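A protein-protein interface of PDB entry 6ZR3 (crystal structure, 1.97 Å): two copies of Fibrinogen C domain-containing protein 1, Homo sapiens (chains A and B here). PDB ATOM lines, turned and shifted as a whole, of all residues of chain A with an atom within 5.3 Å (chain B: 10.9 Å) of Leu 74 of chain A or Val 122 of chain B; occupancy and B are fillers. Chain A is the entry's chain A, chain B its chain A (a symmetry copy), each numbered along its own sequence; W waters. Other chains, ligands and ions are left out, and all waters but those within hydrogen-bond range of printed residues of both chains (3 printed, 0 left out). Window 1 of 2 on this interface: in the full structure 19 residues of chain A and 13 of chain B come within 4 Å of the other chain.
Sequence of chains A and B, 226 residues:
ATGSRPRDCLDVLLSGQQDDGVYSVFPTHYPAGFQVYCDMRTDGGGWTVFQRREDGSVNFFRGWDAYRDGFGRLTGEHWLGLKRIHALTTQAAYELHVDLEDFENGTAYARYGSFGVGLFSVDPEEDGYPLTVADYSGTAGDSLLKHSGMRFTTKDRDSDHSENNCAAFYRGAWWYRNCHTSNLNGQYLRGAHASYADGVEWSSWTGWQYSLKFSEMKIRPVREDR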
ATOM      1  N   VAL A  22       5.955  -2.068 -19.415  1.00  0.00           N
ATOM      2  CA  VAL A  22       6.283  -3.416 -18.885  1.00  0.00           C
ATOM      3  C   VAL A  22       7.185  -3.224 -17.669  1.00  0.00           C
ATOM      4  O   VAL A  22       8.159  -2.455 -17.767  1.00  0.00           O
ATOM      5  CB  VAL A  22       6.938  -4.278 -19.977  1.00  0.00           C
ATOM      6  CG1 VAL A  22       7.495  -5.582 -19.431  1.00  0.00           C
ATOM      7  CG2 VAL A  22       5.966  -4.536 -21.113  1.00  0.00           C
ATOM      8  N   GLN A  35       7.177 -10.343 -15.519  1.00  0.00           N
ATOM      9  CA  GLN A  35       6.907  -9.022 -16.124  1.00  0.00           C
ATOM     10  C   GLN A  35       5.422  -8.939 -16.476  1.00  0.00           C
ATOM     11  O   GLN A  35       4.818  -9.978 -16.830  1.00  0.00           O
ATOM     12  CB  GLN A  35       7.864  -8.792 -17.288  1.00  0.00           C
ATOM     13  CG  GLN A  35       9.303  -8.637 -16.824  1.00  0.00           C
ATOM     14  CD  GLN A  35      10.220  -8.260 -17.960  1.00  0.00           C
ATOM     15  OE1 GLN A  35      10.111  -8.768 -19.068  1.00  0.00           O
ATOM     16  NE2 GLN A  35      11.125  -7.339 -17.696  1.00  0.00           N
ATOM     17  N   VAL A  36       4.857  -7.739 -16.325  1.00  0.00           N
ATOM     18  CA  VAL A  36       3.448  -7.413 -16.667  1.00  0.00           C
ATOM     19  C   VAL A  36       3.428  -6.066 -17.382  1.00  0.00           C
ATOM     20  O   VAL A  36       4.414  -5.289 -17.258  1.00  0.00           O
ATOM     21  CB  VAL A  36       2.576  -7.364 -15.402  1.00  0.00           C
ATOM     22  CG1 VAL A  36       2.515  -8.716 -14.720  1.00  0.00           C
ATOM     23  CG2 VAL A  36       3.059  -6.292 -14.424  1.00  0.00           C
ATOM     24  N   TYR A  37       2.317  -5.773 -18.047  1.00  0.00           N
ATOM     25  CA  TYR A  37       2.000  -4.414 -18.533  1.00  0.00           C
ATOM     26  C   TYR A  37       1.228  -3.660 -17.449  1.00  0.00           C
ATOM     27  O   TYR A  37       0.197  -4.160 -16.999  1.00  0.00           O
ATOM     28  CB  TYR A  37       1.199  -4.441 -19.835  1.00  0.00           C
ATOM     29  CG  TYR A  37       1.302  -3.134 -20.577  1.00  0.00           C
ATOM     30  CD1 TYR A  37       0.510  -2.051 -20.240  1.00  0.00           C
ATOM     31  CD2 TYR A  37       2.241  -2.969 -21.580  1.00  0.00           C
ATOM     32  CE1 TYR A  37       0.627  -0.841 -20.909  1.00  0.00           C
ATOM     33  CE2 TYR A  37       2.376  -1.766 -22.251  1.00  0.00           C
ATOM     34  CZ  TYR A  37       1.568  -0.698 -21.913  1.00  0.00           C
ATOM     35  OH  TYR A  37       1.704   0.475 -22.595  1.00  0.00           O
ATOM     36  N   ARG A  52      -5.543  -8.768 -22.939  1.00  0.00           N
ATOM     37  CA  ARG A  52      -5.700  -7.699 -23.954  1.00  0.00           C
ATOM     38  C   ARG A  52      -6.042  -8.338 -25.302  1.00  0.00           C
ATOM     39  O   ARG A  52      -5.337  -9.274 -25.703  1.00  0.00           O
ATOM     40  CB  ARG A  52      -4.452  -6.827 -24.082  1.00  0.00           C
ATOM     41  CG  ARG A  52      -4.699  -5.623 -24.981  1.00  0.00           C
ATOM     42  CD  ARG A  52      -3.486  -4.770 -25.237  1.00  0.00           C
ATOM     43  NE  ARG A  52      -3.016  -4.145 -24.016  1.00  0.00           N
ATOM     44  CZ  ARG A  52      -1.799  -4.277 -23.492  1.00  0.00           C
ATOM     45  NH1 ARG A  52      -0.880  -5.037 -24.076  1.00  0.00           N
ATOM     46  NH2 ARG A  52      -1.502  -3.627 -22.377  1.00  0.00           N
ATOM     47  N   ASP A  69      -0.467 -21.077 -18.210  1.00  0.00           N
ATOM     48  CA  ASP A  69       0.933 -20.583 -18.286  1.00  0.00           C
ATOM     49  C   ASP A  69       1.025 -19.218 -18.977  1.00  0.00           C
ATOM     50  O   ASP A  69       2.077 -18.586 -18.818  1.00  0.00           O
ATOM     51  CB  ASP A  69       1.837 -21.591 -18.993  1.00  0.00           C
ATOM     52  CG  ASP A  69       2.034 -22.873 -18.205  1.00  0.00           C
ATOM     53  OD1 ASP A  69       1.923 -22.831 -16.957  1.00  0.00           O
ATOM     54  OD2 ASP A  69       2.263 -23.896 -18.844  1.00  0.00           O
ATOM     55  N   GLY A  70      -0.007 -18.795 -19.712  1.00  0.00           N
ATOM     56  CA  GLY A  70      -0.028 -17.513 -20.444  1.00  0.00           C
ATOM     57  C   GLY A  70       0.470 -17.663 -21.873  1.00  0.00           C
ATOM     58  O   GLY A  70       1.146 -18.666 -22.179  1.00  0.00           O
ATOM     59  N   PHE A  71       0.121 -16.705 -22.735  1.00  0.00           N
ATOM     60  CA  PHE A  71       0.520 -16.653 -24.164  1.00  0.00           C
ATOM     61  C   PHE A  71       0.381 -15.213 -24.664  1.00  0.00           C
ATOM     62  O   PHE A  71      -0.187 -14.345 -23.928  1.00  0.00           O
ATOM     63  CB  PHE A  71      -0.301 -17.641 -24.997  1.00  0.00           C
ATOM     64  CG  PHE A  71      -1.794 -17.483 -24.862  1.00  0.00           C
ATOM     65  CD1 PHE A  71      -2.502 -16.625 -25.694  1.00  0.00           C
ATOM     66  CD2 PHE A  71      -2.494 -18.185 -23.893  1.00  0.00           C
ATOM     67  CE1 PHE A  71      -3.873 -16.483 -25.558  1.00  0.00           C
ATOM     68  CE2 PHE A  71      -3.865 -18.046 -23.762  1.00  0.00           C
ATOM     69  CZ  PHE A  71      -4.554 -17.197 -24.599  1.00  0.00           C
ATOM     70  N   GLY A  72       0.902 -14.981 -25.869  1.00  0.00           N
ATOM     71  CA  GLY A  72       0.972 -13.664 -26.510  1.00  0.00           C
ATOM     72  C   GLY A  72       2.087 -12.825 -25.925  1.00  0.00           C
ATOM     73  O   GLY A  72       2.986 -13.384 -25.249  1.00  0.00           O
ATOM     74  N   ARG A  73       2.046 -11.519 -26.183  1.00  0.00           N
ATOM     75  CA  ARG A  73       3.108 -10.568 -25.773  1.00  0.00           C
ATOM     76  C   ARG A  73       2.500  -9.447 -24.928  1.00  0.00           C
ATOM     77  O   ARG A  73       1.401  -8.993 -25.256  1.00  0.00           O
ATOM     78  CB  ARG A  73       3.833 -10.057 -27.019  1.00  0.00           C
ATOM     79  CG  ARG A  73       4.381 -11.207 -27.847  1.00  0.00           C
ATOM     80  CD  ARG A  73       5.503 -10.867 -28.799  1.00  0.00           C
ATOM     81  NE  ARG A  73       5.894 -12.107 -29.463  1.00  0.00           N
ATOM     82  CZ  ARG A  73       6.477 -12.206 -30.655  1.00  0.00           C
ATOM     83  NH1 ARG A  73       6.774 -11.126 -31.357  1.00  0.00           N
ATOM     84  NH2 ARG A  73       6.758 -13.401 -31.145  1.00  0.00           N
ATOM     85  N   LEU A  74       3.253  -8.993 -23.930  1.00  0.00           N
ATOM     86  CA  LEU A  74       2.822  -7.994 -22.920  1.00  0.00           C
ATOM     87  C   LEU A  74       2.489  -6.652 -23.589  1.00  0.00           C
ATOM     88  O   LEU A  74       1.624  -5.941 -23.049  1.00  0.00           O
ATOM     89  CB  LEU A  74       3.937  -7.853 -21.877  1.00  0.00           C
ATOM     90  CG  LEU A  74       4.191  -9.082 -21.008  1.00  0.00           C
ATOM     91  CD1 LEU A  74       5.423  -8.879 -20.141  1.00  0.00           C
ATOM     92  CD2 LEU A  74       2.979  -9.391 -20.143  1.00  0.00           C
ATOM     93  N   THR A  75       3.135  -6.339 -24.719  1.00  0.00           N
ATOM     94  CA  THR A  75       2.993  -5.067 -25.485  1.00  0.00           C
ATOM     95  C   THR A  75       1.827  -5.166 -26.474  1.00  0.00           C
ATOM     96  O   THR A  75       1.472  -4.124 -27.061  1.00  0.00           O
ATOM     97  CB  THR A  75       4.280  -4.721 -26.252  1.00  0.00           C
ATOM     98  OG1 THR A  75       4.755  -5.901 -26.899  1.00  0.00           O
ATOM     99  CG2 THR A  75       5.373  -4.181 -25.358  1.00  0.00           C
ATOM    100  N   GLY A  76       1.248  -6.358 -26.645  1.00  0.00           N
ATOM    101  CA  GLY A  76       0.118  -6.596 -27.560  1.00  0.00           C
ATOM    102  C   GLY A  76      -0.969  -7.452 -26.934  1.00  0.00           C
ATOM    103  O   GLY A  76      -1.249  -7.310 -25.718  1.00  0.00           O
ATOM    104  N   HIS A  78      -2.521 -10.611 -25.263  1.00  0.00           N
ATOM    105  CA  HIS A  78      -1.965 -11.635 -24.351  1.00  0.00           C
ATOM    106  C   HIS A  78      -2.997 -12.054 -23.319  1.00  0.00           C
ATOM    107  O   HIS A  78      -4.030 -11.369 -23.145  1.00  0.00           O
ATOM    108  CB  HIS A  78      -0.660 -11.154 -23.704  1.00  0.00           C
ATOM    109  CG  HIS A  78      -0.795 -10.035 -22.727  1.00  0.00           C
ATOM    110  ND1 HIS A  78      -0.950  -8.712 -23.120  1.00  0.00           N
ATOM    111  CD2 HIS A  78      -0.745 -10.022 -21.376  1.00  0.00           C
ATOM    112  CE1 HIS A  78      -1.009  -7.943 -22.048  1.00  0.00           C
ATOM    113  NE2 HIS A  78      -0.872  -8.713 -20.970  1.00  0.00           N
ATOM    114  N   TRP A  79      -2.687 -13.187 -22.713  1.00  0.00           N
ATOM    115  CA  TRP A  79      -3.302 -13.724 -21.488  1.00  0.00           C
ATOM    116  C   TRP A  79      -2.145 -13.994 -20.532  1.00  0.00           C
ATOM    117  O   TRP A  79      -1.261 -14.756 -20.920  1.00  0.00           O
ATOM    118  CB  TRP A  79      -4.104 -14.975 -21.831  1.00  0.00           C
ATOM    119  CG  TRP A  79      -4.701 -15.638 -20.633  1.00  0.00           C
ATOM    120  CD1 TRP A  79      -4.209 -16.728 -19.981  1.00  0.00           C
ATOM    121  CD2 TRP A  79      -5.894 -15.244 -19.939  1.00  0.00           C
ATOM    122  NE1 TRP A  79      -5.022 -17.050 -18.933  1.00  0.00           N
ATOM    123  CE2 TRP A  79      -6.058 -16.152 -18.873  1.00  0.00           C
ATOM    124  CE3 TRP A  79      -6.846 -14.233 -20.118  1.00  0.00           C
ATOM    125  CZ2 TRP A  79      -7.144 -16.090 -18.004  1.00  0.00           C
ATOM    126  CZ3 TRP A  79      -7.902 -14.153 -19.240  1.00  0.00           C
ATOM    127  CH2 TRP A  79      -8.047 -15.070 -18.198  1.00  0.00           C
ATOM    128  N   LEU A  80      -2.130 -13.354 -19.364  1.00  0.00           N
ATOM    129  CA  LEU A  80      -0.956 -13.390 -18.452  1.00  0.00           C
ATOM    130  C   LEU A  80      -0.791 -14.806 -17.886  1.00  0.00           C
ATOM    131  O   LEU A  80       0.360 -15.176 -17.540  1.00  0.00           O
ATOM    132  CB  LEU A  80      -1.139 -12.342 -17.352  1.00  0.00           C
ATOM    133  CG  LEU A  80       0.008 -12.200 -16.354  1.00  0.00           C
ATOM    134  CD1 LEU A  80       1.269 -11.706 -17.046  1.00  0.00           C
ATOM    135  CD2 LEU A  80      -0.387 -11.253 -15.226  1.00  0.00           C
ATOM    136  N   GLY A  81      -1.875 -15.582 -17.815  1.00  0.00           N
ATOM    137  CA  GLY A  81      -1.822 -16.954 -17.282  1.00  0.00           C
ATOM    138  C   GLY A  81      -2.458 -17.033 -15.908  1.00  0.00           C
ATOM    139  O   GLY A  81      -2.167 -16.172 -15.057  1.00  0.00           O
ATOM    140  N   ARG A  84      -0.387 -16.926 -12.712  1.00  0.00           N
ATOM    141  CA  ARG A  84       0.077 -15.561 -12.360  1.00  0.00           C
ATOM    142  C   ARG A  84      -1.084 -14.739 -11.789  1.00  0.00           C
ATOM    143  O   ARG A  84      -0.852 -14.007 -10.802  1.00  0.00           O
ATOM    144  CB  ARG A  84       0.737 -14.912 -13.574  1.00  0.00           C
ATOM    145  CG  ARG A  84       1.979 -15.663 -14.038  1.00  0.00           C
ATOM    146  CD  ARG A  84       2.756 -14.884 -15.065  1.00  0.00           C
ATOM    147  NE  ARG A  84       3.921 -15.627 -15.503  1.00  0.00           N
ATOM    148  CZ  ARG A  84       3.970 -16.415 -16.560  1.00  0.00           C
ATOM    149  NH1 ARG A  84       2.902 -16.596 -17.325  1.00  0.00           N
ATOM    150  NH2 ARG A  84       5.097 -17.045 -16.845  1.00  0.00           N
ATOM    151  N   HIS B  29      14.582 -12.444 -12.483  1.00  0.00           N
ATOM    152  CA  HIS B  29      13.499 -13.463 -12.481  1.00  0.00           C
ATOM    153  C   HIS B  29      14.066 -14.884 -12.503  1.00  0.00           C
ATOM    154  O   HIS B  29      13.276 -15.805 -12.782  1.00  0.00           O
ATOM    155  CB  HIS B  29      12.506 -13.215 -13.625  1.00  0.00           C
ATOM    156  CG  HIS B  29      11.839 -11.885 -13.508  1.00  0.00           C
ATOM    157  ND1 HIS B  29      11.194 -11.493 -12.354  1.00  0.00           N
ATOM    158  CD2 HIS B  29      11.754 -10.847 -14.367  1.00  0.00           C
ATOM    159  CE1 HIS B  29      10.717 -10.271 -12.518  1.00  0.00           C
ATOM    160  NE2 HIS B  29      11.052  -9.846 -13.747  1.00  0.00           N
ATOM    161  N   HIS B  86      17.105 -15.645 -21.939  1.00  0.00           N
ATOM    162  CA  HIS B  86      15.866 -14.870 -21.675  1.00  0.00           C
ATOM    163  C   HIS B  86      15.961 -14.184 -20.305  1.00  0.00           C
ATOM    164  O   HIS B  86      15.681 -12.970 -20.231  1.00  0.00           O
ATOM    165  CB  HIS B  86      14.623 -15.758 -21.793  1.00  0.00           C
ATOM    166  CG  HIS B  86      13.374 -15.053 -21.400  1.00  0.00           C
ATOM    167  ND1 HIS B  86      12.864 -15.111 -20.109  1.00  0.00           N
ATOM    168  CD2 HIS B  86      12.544 -14.251 -22.101  1.00  0.00           C
ATOM    169  CE1 HIS B  86      11.782 -14.359 -20.037  1.00  0.00           C
ATOM    170  NE2 HIS B  86      11.555 -13.839 -21.252  1.00  0.00           N
ATOM    171  N   THR B  90      16.136  -9.894 -20.521  1.00  0.00           N
ATOM    172  CA  THR B  90      14.880  -9.196 -20.126  1.00  0.00           C
ATOM    173  C   THR B  90      15.078  -8.333 -18.871  1.00  0.00           C
ATOM    174  O   THR B  90      14.157  -7.562 -18.583  1.00  0.00           O
ATOM    175  CB  THR B  90      13.723 -10.164 -19.849  1.00  0.00           C
ATOM    176  OG1 THR B  90      14.173 -11.111 -18.887  1.00  0.00           O
ATOM    177  CG2 THR B  90      13.237 -10.888 -21.080  1.00  0.00           C
ATOM    178  N   VAL B 117      16.074 -12.020 -26.351  1.00  0.00           N
ATOM    179  CA  VAL B 117      15.283 -13.210 -26.777  1.00  0.00           C
ATOM    180  C   VAL B 117      14.005 -13.260 -25.929  1.00  0.00           C
ATOM    181  O   VAL B 117      14.101 -13.168 -24.685  1.00  0.00           O
ATOM    182  CB  VAL B 117      16.106 -14.515 -26.723  1.00  0.00           C
ATOM    183  CG1 VAL B 117      17.452 -14.359 -27.413  1.00  0.00           C
ATOM    184  CG2 VAL B 117      16.307 -15.033 -25.311  1.00  0.00           C
ATOM    185  N   GLY B 118      12.853 -13.373 -26.599  1.00  0.00           N
ATOM    186  CA  GLY B 118      11.519 -13.482 -25.976  1.00  0.00           C
ATOM    187  C   GLY B 118      11.191 -12.287 -25.097  1.00  0.00           C
ATOM    188  O   GLY B 118      10.551 -12.493 -24.056  1.00  0.00           O
ATOM    189  N   LEU B 119      11.601 -11.081 -25.508  1.00  0.00           N
ATOM    190  CA  LEU B 119      11.712  -9.898 -24.607  1.00  0.00           C
ATOM    191  C   LEU B 119      10.379  -9.626 -23.895  1.00  0.00           C
ATOM    192  O   LEU B 119      10.418  -9.301 -22.682  1.00  0.00           O
ATOM    193  CB  LEU B 119      12.202  -8.660 -25.374  1.00  0.00           C
ATOM    194  CG  LEU B 119      13.723  -8.488 -25.487  1.00  0.00           C
ATOM    195  CD1 LEU B 119      14.086  -7.044 -25.801  1.00  0.00           C
ATOM    196  CD2 LEU B 119      14.450  -8.926 -24.224  1.00  0.00           C
ATOM    197  N   PHE B 120       9.259  -9.725 -24.604  1.00  0.00           N
ATOM    198  CA  PHE B 120       7.915  -9.357 -24.084  1.00  0.00           C
ATOM    199  C   PHE B 120       6.955 -10.545 -24.168  1.00  0.00           C
ATOM    200  O   PHE B 120       5.737 -10.344 -24.028  1.00  0.00           O
ATOM    201  CB  PHE B 120       7.354  -8.178 -24.881  1.00  0.00           C
ATOM    202  CG  PHE B 120       8.239  -6.959 -24.901  1.00  0.00           C
ATOM    203  CD1 PHE B 120       8.339  -6.139 -23.787  1.00  0.00           C
ATOM    204  CD2 PHE B 120       8.965  -6.626 -26.034  1.00  0.00           C
ATOM    205  CE1 PHE B 120       9.135  -5.003 -23.809  1.00  0.00           C
ATOM    206  CE2 PHE B 120       9.772  -5.500 -26.051  1.00  0.00           C
ATOM    207  CZ  PHE B 120       9.852  -4.687 -24.941  1.00  0.00           C
ATOM    208  N   SER B 121       7.477 -11.745 -24.410  1.00  0.00           N
ATOM    209  CA  SER B 121       6.692 -13.004 -24.471  1.00  0.00           C
ATOM    210  C   SER B 121       6.193 -13.344 -23.063  1.00  0.00           C
ATOM    211  O   SER B 121       7.031 -13.442 -22.157  1.00  0.00           O
ATOM    212  CB  SER B 121       7.526 -14.134 -25.017  1.00  0.00           C
ATOM    213  OG  SER B 121       8.111 -13.787 -26.261  1.00  0.00           O
ATOM    214  N   VAL B 122       4.895 -13.567 -22.887  1.00  0.00           N
ATOM    215  CA  VAL B 122       4.346 -14.063 -21.588  1.00  0.00           C
ATOM    216  C   VAL B 122       4.959 -15.440 -21.310  1.00  0.00           C
ATOM    217  O   VAL B 122       5.373 -15.691 -20.174  1.00  0.00           O
ATOM    218  CB  VAL B 122       2.810 -14.123 -21.604  1.00  0.00           C
ATOM    219  CG1 VAL B 122       2.281 -14.809 -20.362  1.00  0.00           C
ATOM    220  CG2 VAL B 122       2.197 -12.740 -21.754  1.00  0.00           C
ATOM    221  N   ASP B 123       4.991 -16.301 -22.323  1.00  0.00           N
ATOM    222  CA  ASP B 123       5.624 -17.643 -22.269  1.00  0.00           C
ATOM    223  C   ASP B 123       6.704 -17.686 -23.348  1.00  0.00           C
ATOM    224  O   ASP B 123       6.441 -18.088 -24.473  1.00  0.00           O
ATOM    225  CB  ASP B 123       4.574 -18.750 -22.417  1.00  0.00           C
ATOM    226  CG  ASP B 123       5.114 -20.169 -22.246  1.00  0.00           C
ATOM    227  OD1 ASP B 123       6.344 -20.348 -22.280  1.00  0.00           O
ATOM    228  OD2 ASP B 123       4.294 -21.094 -22.084  1.00  0.00           O
ATOM    229  N   PRO B 124       7.952 -17.267 -23.049  1.00  0.00           N
ATOM    230  CA  PRO B 124       8.996 -17.194 -24.074  1.00  0.00           C
ATOM    231  C   PRO B 124       9.259 -18.538 -24.770  1.00  0.00           C
ATOM    232  O   PRO B 124       9.572 -18.531 -25.950  1.00  0.00           O
ATOM    233  CB  PRO B 124      10.241 -16.704 -23.316  1.00  0.00           C
ATOM    234  CG  PRO B 124       9.938 -16.979 -21.858  1.00  0.00           C
ATOM    235  CD  PRO B 124       8.436 -16.840 -21.725  1.00  0.00           C
ATOM    236  N   GLU B 125       9.091 -19.652 -24.057  1.00  0.00           N
ATOM    237  CA  GLU B 125       9.266 -21.009 -24.636  1.00  0.00           C
ATOM    238  C   GLU B 125       8.186 -21.261 -25.704  1.00  0.00           C
ATOM    239  O   GLU B 125       8.562 -21.531 -26.868  1.00  0.00           O
ATOM    240  CB  GLU B 125       9.257 -22.090 -23.552  1.00  0.00           C
ATOM    241  CG  GLU B 125       9.740 -23.416 -24.103  1.00  0.00           C
ATOM    242  CD  GLU B 125       9.587 -24.649 -23.238  1.00  0.00           C
ATOM    243  OE1 GLU B 125       9.170 -24.523 -22.071  1.00  0.00           O
ATOM    244  OE2 GLU B 125       9.919 -25.732 -23.745  1.00  0.00           O
ATOM    245  N   GLU B 126       6.905 -21.188 -25.327  1.00  0.00           N
ATOM    246  CA  GLU B 126       5.740 -21.311 -26.256  1.00  0.00           C
ATOM    247  C   GLU B 126       5.987 -20.386 -27.454  1.00  0.00           C
ATOM    248  O   GLU B 126       5.880 -20.846 -28.606  1.00  0.00           O
ATOM    249  CB  GLU B 126       4.431 -20.967 -25.531  1.00  0.00           C
ATOM    250  CG  GLU B 126       3.196 -20.854 -26.430  1.00  0.00           C
ATOM    251  CD  GLU B 126       2.795 -19.450 -26.876  1.00  0.00           C
ATOM    252  OE1 GLU B 126       3.028 -18.485 -26.125  1.00  0.00           O
ATOM    253  OE2 GLU B 126       2.261 -19.317 -27.993  1.00  0.00           O
ATOM    254  N   ASP B 127       6.371 -19.140 -27.174  1.00  0.00           N
ATOM    255  CA  ASP B 127       6.505 -18.061 -28.182  1.00  0.00           C
ATOM    256  C   ASP B 127       7.758 -18.278 -29.046  1.00  0.00           C
ATOM    257  O   ASP B 127       7.911 -17.522 -30.010  1.00  0.00           O
ATOM    258  CB  ASP B 127       6.523 -16.700 -27.485  1.00  0.00           C
ATOM    259  CG  ASP B 127       6.135 -15.543 -28.380  1.00  0.00           C
ATOM    260  OD1 ASP B 127       5.393 -15.787 -29.348  1.00  0.00           O
ATOM    261  OD2 ASP B 127       6.596 -14.409 -28.110  1.00  0.00           O
ATOM    262  N   GLY B 128       8.635 -19.233 -28.698  1.00  0.00           N
ATOM    263  CA  GLY B 128       9.811 -19.633 -29.503  1.00  0.00           C
ATOM    264  C   GLY B 128      11.008 -18.689 -29.359  1.00  0.00           C
ATOM    265  O   GLY B 128      11.820 -18.598 -30.322  1.00  0.00           O
ATOM    266  N   TYR B 129      11.137 -18.008 -28.216  1.00  0.00           N
ATOM    267  CA  TYR B 129      12.292 -17.142 -27.859  1.00  0.00           C
ATOM    268  C   TYR B 129      12.656 -16.237 -29.030  1.00  0.00           C
ATOM    269  O   TYR B 129      13.795 -16.238 -29.480  1.00  0.00           O
ATOM    270  CB  TYR B 129      13.499 -17.995 -27.467  1.00  0.00           C
ATOM    271  CG  TYR B 129      13.292 -18.842 -26.237  1.00  0.00           C
ATOM    272  CD1 TYR B 129      13.297 -18.276 -24.972  1.00  0.00           C
ATOM    273  CD2 TYR B 129      13.075 -20.204 -26.336  1.00  0.00           C
ATOM    274  CE1 TYR B 129      13.099 -19.044 -23.836  1.00  0.00           C
ATOM    275  CE2 TYR B 129      12.873 -20.985 -25.211  1.00  0.00           C
ATOM    276  CZ  TYR B 129      12.875 -20.402 -23.955  1.00  0.00           C
ATOM    277  OH  TYR B 129      12.683 -21.166 -22.840  1.00  0.00           O
ATOM    278  N   PRO B 130      11.715 -15.430 -29.562  1.00  0.00           N
ATOM    279  CA  PRO B 130      11.989 -14.629 -30.753  1.00  0.00           C
ATOM    280  C   PRO B 130      13.142 -13.635 -30.556  1.00  0.00           C
ATOM    281  O   PRO B 130      13.266 -13.070 -29.483  1.00  0.00           O
ATOM    282  CB  PRO B 130      10.662 -13.902 -31.023  1.00  0.00           C
ATOM    283  CG  PRO B 130       9.937 -13.933 -29.699  1.00  0.00           C
ATOM    284  CD  PRO B 130      10.344 -15.247 -29.063  1.00  0.00           C
ATOM    285  N   ARG B 151      11.456 -16.474 -34.616  1.00  0.00           N
ATOM    286  CA  ARG B 151      11.460 -17.467 -33.514  1.00  0.00           C
ATOM    287  C   ARG B 151      12.667 -18.390 -33.721  1.00  0.00           C
ATOM    288  O   ARG B 151      13.209 -18.448 -34.839  1.00  0.00           O
ATOM    289  CB  ARG B 151      10.115 -18.197 -33.460  1.00  0.00           C
ATOM    290  CG  ARG B 151       8.939 -17.269 -33.186  1.00  0.00           C
ATOM    291  CD  ARG B 151       7.649 -18.038 -32.979  1.00  0.00           C
ATOM    292  NE  ARG B 151       6.648 -17.316 -32.198  1.00  0.00           N
ATOM    293  CZ  ARG B 151       5.537 -16.757 -32.675  1.00  0.00           C
ATOM    294  NH1 ARG B 151       5.251 -16.797 -33.968  1.00  0.00           N
ATOM    295  NH2 ARG B 151       4.708 -16.143 -31.848  1.00  0.00           N
HETATM  296  O   HOH W   1       4.561 -18.537 -18.957  1.00  0.00           O
HETATM  297  O   HOH W   2       1.748 -21.234 -22.804  1.00  0.00           O
HETATM  298  O   HOH W   3       4.150 -15.830 -25.054  1.00  0.00           O
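No position is printed for both chains.
N of Leu 74 of chain A is in hydrogen-bond range of O of Phe 120 of chain B (2.8 Å). The backbone carbonyl oxygen (O) of Gly 72 of chain A is in hydrogen-bond range of the backbone NH (N) of Val 122 of chain B. The guanidinium group of Arg 73 of chain A lies within salt-bridge range of the side-chain carboxylate of Asp 127 of chain B, 2.8 Å away. NH2 of Arg 73 of chain A lies close to NH2 of Arg 151 of chain B (3.5 Å). The backbone carbonyl oxygen of Thr 90 of chain B lies within hydrogen-bond range of the side-chain amide nitrogen of Gln 35 of chain A (3.2 Å).
Among the printed residues, merely in contact across the chains: Val 22 of chain A with Phe 120 of chain B (3.9 Å), Gln 35 of chain A with His 29 of chain B (3.7 Å), Gln 35 of chain A with Leu 119 of chain B (3.7 Å), Asp 69 of chain A with Asp 123 of chain B (3.98 Å), Gly 70 of chain A with Val 122 of chain B (3.6 Å), Gly 70 of chain A with Asp 123 of chain B (3.4 Å), Phe 71 of chain A with Val 122 of chain B (3.6 Å), Phe 71 of chain A with Glu 126 of chain B (3.6 Å), Gly 72 of chain A with Ser 121 of chain B (3.8 Å), Arg 73 of chain A with Phe 120 of chain B (3.2 Å), Arg 73 of chain A with Pro 130 of chain B (3.5 Å), Leu 74 of chain A with Val 122 of chain B (3.8 Å), Thr 75 of chain A with Phe 120 of chain B (3.9 Å), His 78 of chain A with Val 122 of chain B (3.8 Å), Trp 79 of chain A with Val 122 of chain B (3.6 Å), Leu 80 of chain A with Val 122 of chain B (3.4 Å) and Arg 84 of chain A with Val 122 of chain B (3.6 Å).
NH1 of Arg 52 of chain A lies within hydrogen-bond range of O of Leu 74 of chain A (2.9 Å). The side-chain hydroxyl of Ser 121 of chain B lies within hydrogen-bond range of the side-chain carboxylate of Asp 127 of chain B (2.5 Å).
Of chain B, only His 29, Thr 90 and Leu 119 come within 4 Å of Gln 35 of chain A. No residue of chain B comes within 4 Å of Val 36 of chain A. No residue of chain B comes within 4 Å of Tyr 37 of chain A. Printed residues of chain B within 4 Å of Phe 71 of chain A: Val 122 (3.6 Å) and Glu 126 (3.6 Å). Gly 72 of chain A touches just these residues of chain B: Ser 121 (3.8 Å) and Val 122 (3.0 Å). Of chain B, only Phe 120 comes within 4 Å of Thr 75 of chain A. Of the printed residues of chain B, Leu 80 of chain A touches Val 122 (3.4 Å). Pro 124 of chain B touches none of the printed residues of chain A. Printed residues of chain A within 4 Å of Arg 151 of chain B: Arg 73. The nearest printed residue of chain A that does not touch Asp 123 of chain B is Gly 72 of chain A (4.6 Å).
Water W1 lies within hydrogen-bond range of O of Asp 69 of chain A (2.5 Å), NH2 of Arg 84 of chain A (2.6 Å) and O of Val 122 of chain B (3.2 Å). Water W2 lies within hydrogen-bond range of the side-chain carboxylate of Asp 123 of chain B (2.6 Å) and the backbone carbonyl oxygen of Gly 70 of chain A (2.7 Å).
Hydrophobic or aromatic side chains of chain B within 4 Å of the printed part of chain A: His 29, Phe 120, Val 122 and Pro 130. Of the 18 printed residues of chain A, 13 touch a printed residue of chain B. Among the printed residues, Asp or Glu carboxylates within 4 Å of a Lys or Arg side-chain nitrogen of the other chain: Arg 73 of chain A with Asp 127 of chain B.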
